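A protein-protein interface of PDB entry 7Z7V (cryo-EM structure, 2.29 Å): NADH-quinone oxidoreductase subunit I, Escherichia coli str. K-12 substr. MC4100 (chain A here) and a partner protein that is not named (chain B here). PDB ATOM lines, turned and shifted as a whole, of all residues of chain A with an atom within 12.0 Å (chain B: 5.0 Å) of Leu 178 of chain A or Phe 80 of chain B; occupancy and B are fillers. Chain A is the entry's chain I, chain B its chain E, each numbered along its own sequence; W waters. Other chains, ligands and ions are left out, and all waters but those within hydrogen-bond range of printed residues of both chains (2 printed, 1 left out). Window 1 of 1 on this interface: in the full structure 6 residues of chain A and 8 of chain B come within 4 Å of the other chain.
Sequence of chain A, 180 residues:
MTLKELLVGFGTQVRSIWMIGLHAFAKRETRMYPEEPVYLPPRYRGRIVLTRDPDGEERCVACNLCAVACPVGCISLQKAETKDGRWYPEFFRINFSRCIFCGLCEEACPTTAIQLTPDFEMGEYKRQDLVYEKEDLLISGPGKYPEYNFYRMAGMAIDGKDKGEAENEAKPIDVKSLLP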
ATOM      1  N   PRO A 172     -28.884  32.458   5.640  1.00  0.00           N
ATOM      2  CA  PRO A 172     -28.948  31.151   6.306  1.00  0.00           C
ATOM      3  C   PRO A 172     -27.936  31.054   7.438  1.00  0.00           C
ATOM      4  O   PRO A 172     -26.777  31.444   7.291  1.00  0.00           O
ATOM      5  CB  PRO A 172     -28.640  30.157   5.180  1.00  0.00           C
ATOM      6  CG  PRO A 172     -27.980  30.958   4.125  1.00  0.00           C
ATOM      7  CD  PRO A 172     -28.540  32.333   4.214  1.00  0.00           C
ATOM      8  N   ILE A 173     -28.393  30.543   8.573  1.00  0.00           N
ATOM      9  CA  ILE A 173     -27.560  30.345   9.753  1.00  0.00           C
ATOM     10  C   ILE A 173     -27.292  28.856   9.876  1.00  0.00           C
ATOM     11  O   ILE A 173     -28.227  28.061  10.022  1.00  0.00           O
ATOM     12  CB  ILE A 173     -28.229  30.890  11.023  1.00  0.00           C
ATOM     13  CG1 ILE A 173     -28.443  32.398  10.913  1.00  0.00           C
ATOM     14  CG2 ILE A 173     -27.398  30.551  12.251  1.00  0.00           C
ATOM     15  CD1 ILE A 173     -29.561  32.912  11.779  1.00  0.00           C
ATOM     16  N   ASP A 174     -26.020  28.480   9.804  1.00  0.00           N
ATOM     17  CA  ASP A 174     -25.641  27.085   9.943  1.00  0.00           C
ATOM     18  C   ASP A 174     -25.904  26.607  11.366  1.00  0.00           C
ATOM     19  O   ASP A 174     -25.770  27.361  12.331  1.00  0.00           O
ATOM     20  CB  ASP A 174     -24.167  26.898   9.585  1.00  0.00           C
ATOM     21  CG  ASP A 174     -23.847  25.483   9.152  1.00  0.00           C
ATOM     22  OD1 ASP A 174     -23.497  25.286   7.972  1.00  0.00           O
ATOM     23  OD2 ASP A 174     -23.942  24.565   9.989  1.00  0.00           O
ATOM     24  N   VAL A 175     -26.291  25.335  11.488  1.00  0.00           N
ATOM     25  CA  VAL A 175     -26.513  24.753  12.807  1.00  0.00           C
ATOM     26  C   VAL A 175     -25.211  24.591  13.575  1.00  0.00           C
ATOM     27  O   VAL A 175     -25.235  24.432  14.799  1.00  0.00           O
ATOM     28  CB  VAL A 175     -27.237  23.400  12.696  1.00  0.00           C
ATOM     29  CG1 VAL A 175     -28.672  23.607  12.262  1.00  0.00           C
ATOM     30  CG2 VAL A 175     -26.504  22.479  11.741  1.00  0.00           C
ATOM     31  N   LYS A 176     -24.075  24.641  12.888  1.00  0.00           N
ATOM     32  CA  LYS A 176     -22.763  24.562  13.509  1.00  0.00           C
ATOM     33  C   LYS A 176     -22.239  25.919  13.960  1.00  0.00           C
ATOM     34  O   LYS A 176     -21.092  26.003  14.406  1.00  0.00           O
ATOM     35  CB  LYS A 176     -21.768  23.925  12.536  1.00  0.00           C
ATOM     36  CG  LYS A 176     -21.986  22.441  12.323  1.00  0.00           C
ATOM     37  CD  LYS A 176     -21.730  22.043  10.888  1.00  0.00           C
ATOM     38  CE  LYS A 176     -20.251  22.056  10.575  1.00  0.00           C
ATOM     39  NZ  LYS A 176     -19.973  22.672   9.249  1.00  0.00           N
ATOM     40  N   SER A 177     -23.040  26.976  13.851  1.00  0.00           N
ATOM     41  CA  SER A 177     -22.587  28.310  14.217  1.00  0.00           C
ATOM     42  C   SER A 177     -22.431  28.441  15.727  1.00  0.00           C
ATOM     43  O   SER A 177     -23.165  27.833  16.509  1.00  0.00           O
ATOM     44  CB  SER A 177     -23.559  29.369  13.700  1.00  0.00           C
ATOM     45  OG  SER A 177     -24.601  29.607  14.626  1.00  0.00           O
ATOM     46  N   LEU A 178     -21.455  29.256  16.132  1.00  0.00           N
ATOM     47  CA  LEU A 178     -21.124  29.398  17.545  1.00  0.00           C
ATOM     48  C   LEU A 178     -22.121  30.260  18.304  1.00  0.00           C
ATOM     49  O   LEU A 178     -22.172  30.181  19.534  1.00  0.00           O
ATOM     50  CB  LEU A 178     -19.724  29.988  17.698  1.00  0.00           C
ATOM     51  CG  LEU A 178     -18.617  29.351  16.861  1.00  0.00           C
ATOM     52  CD1 LEU A 178     -17.398  30.251  16.826  1.00  0.00           C
ATOM     53  CD2 LEU A 178     -18.263  27.986  17.414  1.00  0.00           C
ATOM     54  N   LEU A 179     -22.898  31.078  17.613  1.00  0.00           N
ATOM     55  CA  LEU A 179     -23.835  31.965  18.289  1.00  0.00           C
ATOM     56  C   LEU A 179     -25.004  31.161  18.846  1.00  0.00           C
ATOM     57  O   LEU A 179     -25.545  30.301  18.144  1.00  0.00           O
ATOM     58  CB  LEU A 179     -24.333  33.039  17.328  1.00  0.00           C
ATOM     59  CG  LEU A 179     -23.341  34.169  17.055  1.00  0.00           C
ATOM     60  CD1 LEU A 179     -23.881  35.115  16.003  1.00  0.00           C
ATOM     61  CD2 LEU A 179     -23.027  34.916  18.337  1.00  0.00           C
ATOM     62  N   PRO A 180     -25.421  31.406  20.099  1.00  0.00           N
ATOM     63  CA  PRO A 180     -26.497  30.657  20.761  1.00  0.00           C
ATOM     64  C   PRO A 180     -27.859  30.836  20.091  1.00  0.00           C
ATOM     65  O   PRO A 180     -28.131  31.902  19.541  1.00  0.00           O
ATOM     66  CB  PRO A 180     -26.517  31.242  22.179  1.00  0.00           C
ATOM     67  CG  PRO A 180     -25.242  32.002  22.321  1.00  0.00           C
ATOM     68  CD  PRO A 180     -24.895  32.476  20.960  1.00  0.00           C
ATOM     69  N   GLN B  44     -13.550  18.367  22.605  1.00  0.00           N
ATOM     70  CA  GLN B  44     -13.432  19.821  22.573  1.00  0.00           C
ATOM     71  C   GLN B  44     -12.344  20.320  23.515  1.00  0.00           C
ATOM     72  O   GLN B  44     -11.608  21.251  23.180  1.00  0.00           O
ATOM     73  CB  GLN B  44     -14.776  20.457  22.923  1.00  0.00           C
ATOM     74  CG  GLN B  44     -14.747  21.966  23.004  1.00  0.00           C
ATOM     75  CD  GLN B  44     -16.122  22.577  22.941  1.00  0.00           C
ATOM     76  OE1 GLN B  44     -16.799  22.499  21.920  1.00  0.00           O
ATOM     77  NE2 GLN B  44     -16.546  23.195  24.035  1.00  0.00           N
ATOM     78  N   GLY B  48      -9.924  22.149  21.312  1.00  0.00           N
ATOM     79  CA  GLY B  48     -10.542  23.454  21.198  1.00  0.00           C
ATOM     80  C   GLY B  48     -11.966  23.433  20.678  1.00  0.00           C
ATOM     81  O   GLY B  48     -12.780  24.265  21.086  1.00  0.00           O
ATOM     82  N   TRP B  49     -12.283  22.497  19.790  1.00  0.00           N
ATOM     83  CA  TRP B  49     -13.611  22.364  19.213  1.00  0.00           C
ATOM     84  C   TRP B  49     -13.786  20.914  18.783  1.00  0.00           C
ATOM     85  O   TRP B  49     -12.879  20.093  18.924  1.00  0.00           O
ATOM     86  CB  TRP B  49     -13.808  23.336  18.044  1.00  0.00           C
ATOM     87  CG  TRP B  49     -12.956  23.038  16.845  1.00  0.00           C
ATOM     88  CD1 TRP B  49     -11.595  23.025  16.789  1.00  0.00           C
ATOM     89  CD2 TRP B  49     -13.414  22.722  15.527  1.00  0.00           C
ATOM     90  NE1 TRP B  49     -11.176  22.713  15.523  1.00  0.00           N
ATOM     91  CE2 TRP B  49     -12.274  22.523  14.727  1.00  0.00           C
ATOM     92  CE3 TRP B  49     -14.676  22.582  14.946  1.00  0.00           C
ATOM     93  CZ2 TRP B  49     -12.358  22.194  13.380  1.00  0.00           C
ATOM     94  CZ3 TRP B  49     -14.758  22.259  13.610  1.00  0.00           C
ATOM     95  CH2 TRP B  49     -13.607  22.068  12.840  1.00  0.00           C
ATOM     96  N   VAL B  50     -14.963  20.600  18.255  1.00  0.00           N
ATOM     97  CA  VAL B  50     -15.274  19.254  17.795  1.00  0.00           C
ATOM     98  C   VAL B  50     -15.262  19.271  16.267  1.00  0.00           C
ATOM     99  O   VAL B  50     -16.195  19.801  15.650  1.00  0.00           O
ATOM    100  CB  VAL B  50     -16.624  18.765  18.334  1.00  0.00           C
ATOM    101  CG1 VAL B  50     -16.913  17.366  17.835  1.00  0.00           C
ATOM    102  CG2 VAL B  50     -16.639  18.807  19.849  1.00  0.00           C
ATOM    103  N   SER B  77     -25.036  24.686  23.032  1.00  0.00           N
ATOM    104  CA  SER B  77     -24.327  25.863  22.542  1.00  0.00           C
ATOM    105  C   SER B  77     -22.851  25.844  22.913  1.00  0.00           C
ATOM    106  O   SER B  77     -22.034  26.439  22.205  1.00  0.00           O
ATOM    107  CB  SER B  77     -24.991  27.130  23.075  1.00  0.00           C
ATOM    108  OG  SER B  77     -25.302  27.007  24.448  1.00  0.00           O
ATOM    109  N   GLN B  78     -22.486  25.176  23.999  1.00  0.00           N
ATOM    110  CA  GLN B  78     -21.102  25.168  24.448  1.00  0.00           C
ATOM    111  C   GLN B  78     -20.270  24.068  23.808  1.00  0.00           C
ATOM    112  O   GLN B  78     -19.069  23.986  24.077  1.00  0.00           O
ATOM    113  CB  GLN B  78     -21.040  25.050  25.971  1.00  0.00           C
ATOM    114  CG  GLN B  78     -21.644  26.238  26.696  1.00  0.00           C
ATOM    115  CD  GLN B  78     -21.308  27.561  26.032  1.00  0.00           C
ATOM    116  OE1 GLN B  78     -20.140  27.915  25.885  1.00  0.00           O
ATOM    117  NE2 GLN B  78     -22.333  28.301  25.636  1.00  0.00           N
ATOM    118  N   ILE B  79     -20.870  23.223  22.979  1.00  0.00           N
ATOM    119  CA  ILE B  79     -20.120  22.294  22.145  1.00  0.00           C
ATOM    120  C   ILE B  79     -19.906  22.981  20.804  1.00  0.00           C
ATOM    121  O   ILE B  79     -20.859  23.238  20.067  1.00  0.00           O
ATOM    122  CB  ILE B  79     -20.849  20.956  21.988  1.00  0.00           C
ATOM    123  CG1 ILE B  79     -20.906  20.232  23.333  1.00  0.00           C
ATOM    124  CG2 ILE B  79     -20.162  20.097  20.946  1.00  0.00           C
ATOM    125  CD1 ILE B  79     -21.992  19.199  23.421  1.00  0.00           C
ATOM    126  N   PHE B  80     -18.653  23.296  20.495  1.00  0.00           N
ATOM    127  CA  PHE B  80     -18.323  24.110  19.335  1.00  0.00           C
ATOM    128  C   PHE B  80     -18.066  23.214  18.132  1.00  0.00           C
ATOM    129  O   PHE B  80     -17.163  22.374  18.155  1.00  0.00           O
ATOM    130  CB  PHE B  80     -17.111  24.990  19.622  1.00  0.00           C
ATOM    131  CG  PHE B  80     -17.307  25.925  20.775  1.00  0.00           C
ATOM    132  CD1 PHE B  80     -18.494  26.618  20.923  1.00  0.00           C
ATOM    133  CD2 PHE B  80     -16.307  26.112  21.710  1.00  0.00           C
ATOM    134  CE1 PHE B  80     -18.679  27.482  21.982  1.00  0.00           C
ATOM    135  CE2 PHE B  80     -16.486  26.973  22.768  1.00  0.00           C
ATOM    136  CZ  PHE B  80     -17.675  27.657  22.906  1.00  0.00           C
ATOM    137  N   ARG B  81     -18.865  23.395  17.087  1.00  0.00           N
ATOM    138  CA  ARG B  81     -18.708  22.663  15.843  1.00  0.00           C
ATOM    139  C   ARG B  81     -18.046  23.501  14.760  1.00  0.00           C
ATOM    140  O   ARG B  81     -17.999  23.083  13.601  1.00  0.00           O
ATOM    141  CB  ARG B  81     -20.065  22.149  15.372  1.00  0.00           C
ATOM    142  CG  ARG B  81     -20.568  20.970  16.178  1.00  0.00           C
ATOM    143  CD  ARG B  81     -19.722  19.744  15.922  1.00  0.00           C
ATOM    144  NE  ARG B  81     -20.033  19.149  14.629  1.00  0.00           N
ATOM    145  CZ  ARG B  81     -19.238  19.190  13.570  1.00  0.00           C
ATOM    146  NH1 ARG B  81     -18.053  19.770  13.618  1.00  0.00           N
ATOM    147  NH2 ARG B  81     -19.644  18.631  12.435  1.00  0.00           N
ATOM    148  N   GLN B  82     -17.545  24.677  15.114  1.00  0.00           N
ATOM    149  CA  GLN B  82     -16.740  25.532  14.264  1.00  0.00           C
ATOM    150  C   GLN B  82     -15.466  25.881  15.014  1.00  0.00           C
ATOM    151  O   GLN B  82     -15.469  25.918  16.247  1.00  0.00           O
ATOM    152  CB  GLN B  82     -17.496  26.811  13.884  1.00  0.00           C
ATOM    153  CG  GLN B  82     -18.238  26.707  12.570  1.00  0.00           C
ATOM    154  CD  GLN B  82     -19.282  27.785  12.401  1.00  0.00           C
ATOM    155  OE1 GLN B  82     -19.253  28.806  13.085  1.00  0.00           O
ATOM    156  NE2 GLN B  82     -20.213  27.566  11.482  1.00  0.00           N
ATOM    157  N   PRO B  83     -14.355  26.099  14.306  1.00  0.00           N
ATOM    158  CA  PRO B  83     -13.095  26.400  14.997  1.00  0.00           C
ATOM    159  C   PRO B  83     -13.157  27.723  15.744  1.00  0.00           C
ATOM    160  O   PRO B  83     -13.683  28.719  15.247  1.00  0.00           O
ATOM    161  CB  PRO B  83     -12.066  26.439  13.861  1.00  0.00           C
ATOM    162  CG  PRO B  83     -12.857  26.613  12.622  1.00  0.00           C
ATOM    163  CD  PRO B  83     -14.154  25.925  12.859  1.00  0.00           C
ATOM    164  N   VAL B  84     -12.619  27.715  16.959  1.00  0.00           N
ATOM    165  CA  VAL B  84     -12.621  28.878  17.828  1.00  0.00           C
ATOM    166  C   VAL B  84     -11.179  29.298  18.075  1.00  0.00           C
ATOM    167  O   VAL B  84     -10.232  28.636  17.651  1.00  0.00           O
ATOM    168  CB  VAL B  84     -13.352  28.616  19.158  1.00  0.00           C
ATOM    169  CG1 VAL B  84     -14.817  28.326  18.908  1.00  0.00           C
ATOM    170  CG2 VAL B  84     -12.698  27.473  19.910  1.00  0.00           C
ATOM    171  N   VAL B  88     -11.821  31.633  24.691  1.00  0.00           N
ATOM    172  CA  VAL B  88     -13.220  31.934  24.422  1.00  0.00           C
ATOM    173  C   VAL B  88     -13.705  32.889  25.502  1.00  0.00           C
ATOM    174  O   VAL B  88     -13.795  32.518  26.675  1.00  0.00           O
ATOM    175  CB  VAL B  88     -14.076  30.663  24.380  1.00  0.00           C
ATOM    176  CG1 VAL B  88     -15.473  30.983  23.880  1.00  0.00           C
ATOM    177  CG2 VAL B  88     -13.420  29.606  23.511  1.00  0.00           C
ATOM    178  N   GLY B 118     -19.410  36.314  18.068  1.00  0.00           N
ATOM    179  CA  GLY B 118     -19.436  35.143  17.224  1.00  0.00           C
ATOM    180  C   GLY B 118     -18.243  34.993  16.308  1.00  0.00           C
ATOM    181  O   GLY B 118     -18.147  33.980  15.607  1.00  0.00           O
ATOM    182  N   THR B 127     -12.001  34.457  20.787  1.00  0.00           N
ATOM    183  CA  THR B 127     -13.303  34.419  20.137  1.00  0.00           C
ATOM    184  C   THR B 127     -14.339  34.967  21.106  1.00  0.00           C
ATOM    185  O   THR B 127     -14.391  34.556  22.269  1.00  0.00           O
ATOM    186  CB  THR B 127     -13.665  33.003  19.663  1.00  0.00           C
ATOM    187  OG1 THR B 127     -15.061  32.935  19.351  1.00  0.00           O
ATOM    188  CG2 THR B 127     -13.320  31.975  20.704  1.00  0.00           C
ATOM    189  N   LEU B 129     -18.147  35.709  22.408  1.00  0.00           N
ATOM    190  CA  LEU B 129     -19.440  35.070  22.370  1.00  0.00           C
ATOM    191  C   LEU B 129     -20.341  35.648  23.455  1.00  0.00           C
ATOM    192  O   LEU B 129     -19.913  35.769  24.621  1.00  0.00           O
ATOM    193  CB  LEU B 129     -19.313  33.555  22.552  1.00  0.00           C
ATOM    194  CG  LEU B 129     -18.758  32.729  21.392  1.00  0.00           C
ATOM    195  CD1 LEU B 129     -18.610  31.278  21.807  1.00  0.00           C
ATOM    196  CD2 LEU B 129     -19.638  32.855  20.166  1.00  0.00           C
HETATM  197  O   HOH W   1     -22.591  29.305  21.933  1.00  0.00           O
HETATM  198  O   HOH W   2     -20.954  25.395  17.107  1.00  0.00           O
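Water W1 bridges O of Leu 178 of chain A (2.6 Å) and O of Ser 77 of chain B (2.9 Å). Water W2 lies within hydrogen-bond range of the backbone carbonyl oxygen of Lys 176 of chain A (2.8 Å), the backbone NH of Arg 81 of chain B (2.9 Å) and the backbone carbonyl oxygen of Ser 177 of chain A (3.3 Å).
N of Phe 80 of chain B lies within hydrogen-bond range of OE1 of Gln 44 of chain B, 2.5 Å away. The backbone NH (N) of Val 50 of chain B lies within hydrogen-bond range of the backbone carbonyl oxygen (O) of Phe 80 of chain B, 2.8 Å away. The backbone carbonyl oxygen (O) of Val 50 of chain B is in hydrogen-bond range of the guanidinium group (NH1) of Arg 81 of chain B (2.8 Å). N of Lys 176 of chain A lies within hydrogen-bond range of OD2 of Asp 174 of chain A (2.9 Å). O of Asp 174 of chain A lies close to OG of Ser 177 of chain A, at 3.4 Å.
Hydrophobic or aromatic side chains of chain A that line the printed part of chain B: Leu 178 and Leu 179. Printed residues of chain B that touch a printed residue of chain A: Phe 80, Arg 81, Gln 82, Val 84, Gly 118 and Leu 129. Among the printed residues, no Asp or Glu carboxylate lies within 4 Å of a Lys or Arg side-chain nitrogen of the other chain.
Printed residues of chain B within 4 Å of Leu 178 of chain A: Phe 80, Gln 82, Val 84, Gly 118 and Leu 129. Phe 80 of chain B touches just one residue of chain A: Leu 178. Gln 44 of chain B touches none of the printed residues of chain A. No residue of chain A comes within 4 Å of Gly 48 of chain B. No residue of chain A comes within 4 Å of Ser 77 of chain B. No residue of chain A comes within 4 Å of Gln 78 of chain B. Of chain A, only Lys 176 comes within 4 Å of Arg 81 of chain B. Gln 82 of chain B touches three residues of chain A. No residue of chain A comes within 4 Å of Val 88 of chain B. Of the printed residues of chain A, Gly 118 of chain B touches Leu 178 (3.99 Å) and Leu 179 (3.8 Å). Printed residues of chain B within 4 Å of Leu 179 of chain A: Gly 118. Val 175 of chain A touches none of the printed residues of chain B. The nearest printed residue of chain B that does not touch Leu 178 of chain A is Pro 83 of chain B (4.3 Å). The nearest residue of chain A that does not touch Phe 80 of chain B is Lys 176 of chain A (5.6 Å). The nearest printed residue of chain B that does not touch Ser 177 of chain A is Arg 81 of chain B (5.9 Å).
Lys 176 of chain A touches Arg 81 of chain B. Gln 82 of chain B touches Ser 177 of chain A (OE1 to CA, 3.6 Å). CD1 of Phe 80 of chain B touches CD2 of Leu 178 of chain A, at 3.8 Å. CD2 of Leu 178 of chain A touches O of Gln 82 of chain B, 3.7 Å away. CG1 of Val 84 of chain B touches CD2 of Leu 178 of chain A, at 3.8 Å. O of Gly 118 of chain B touches CD1 of Leu 178 of chain A (3.99 Å). Leu 178 of chain A touches Leu 129 of chain B. CD2 of Leu 179 of chain A touches CA of Gly 118 of chain B, 3.8 Å away.
NE2 of Gln 82 of chain B lies close to O of Lys 176 of chain A, at 3.4 Å.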
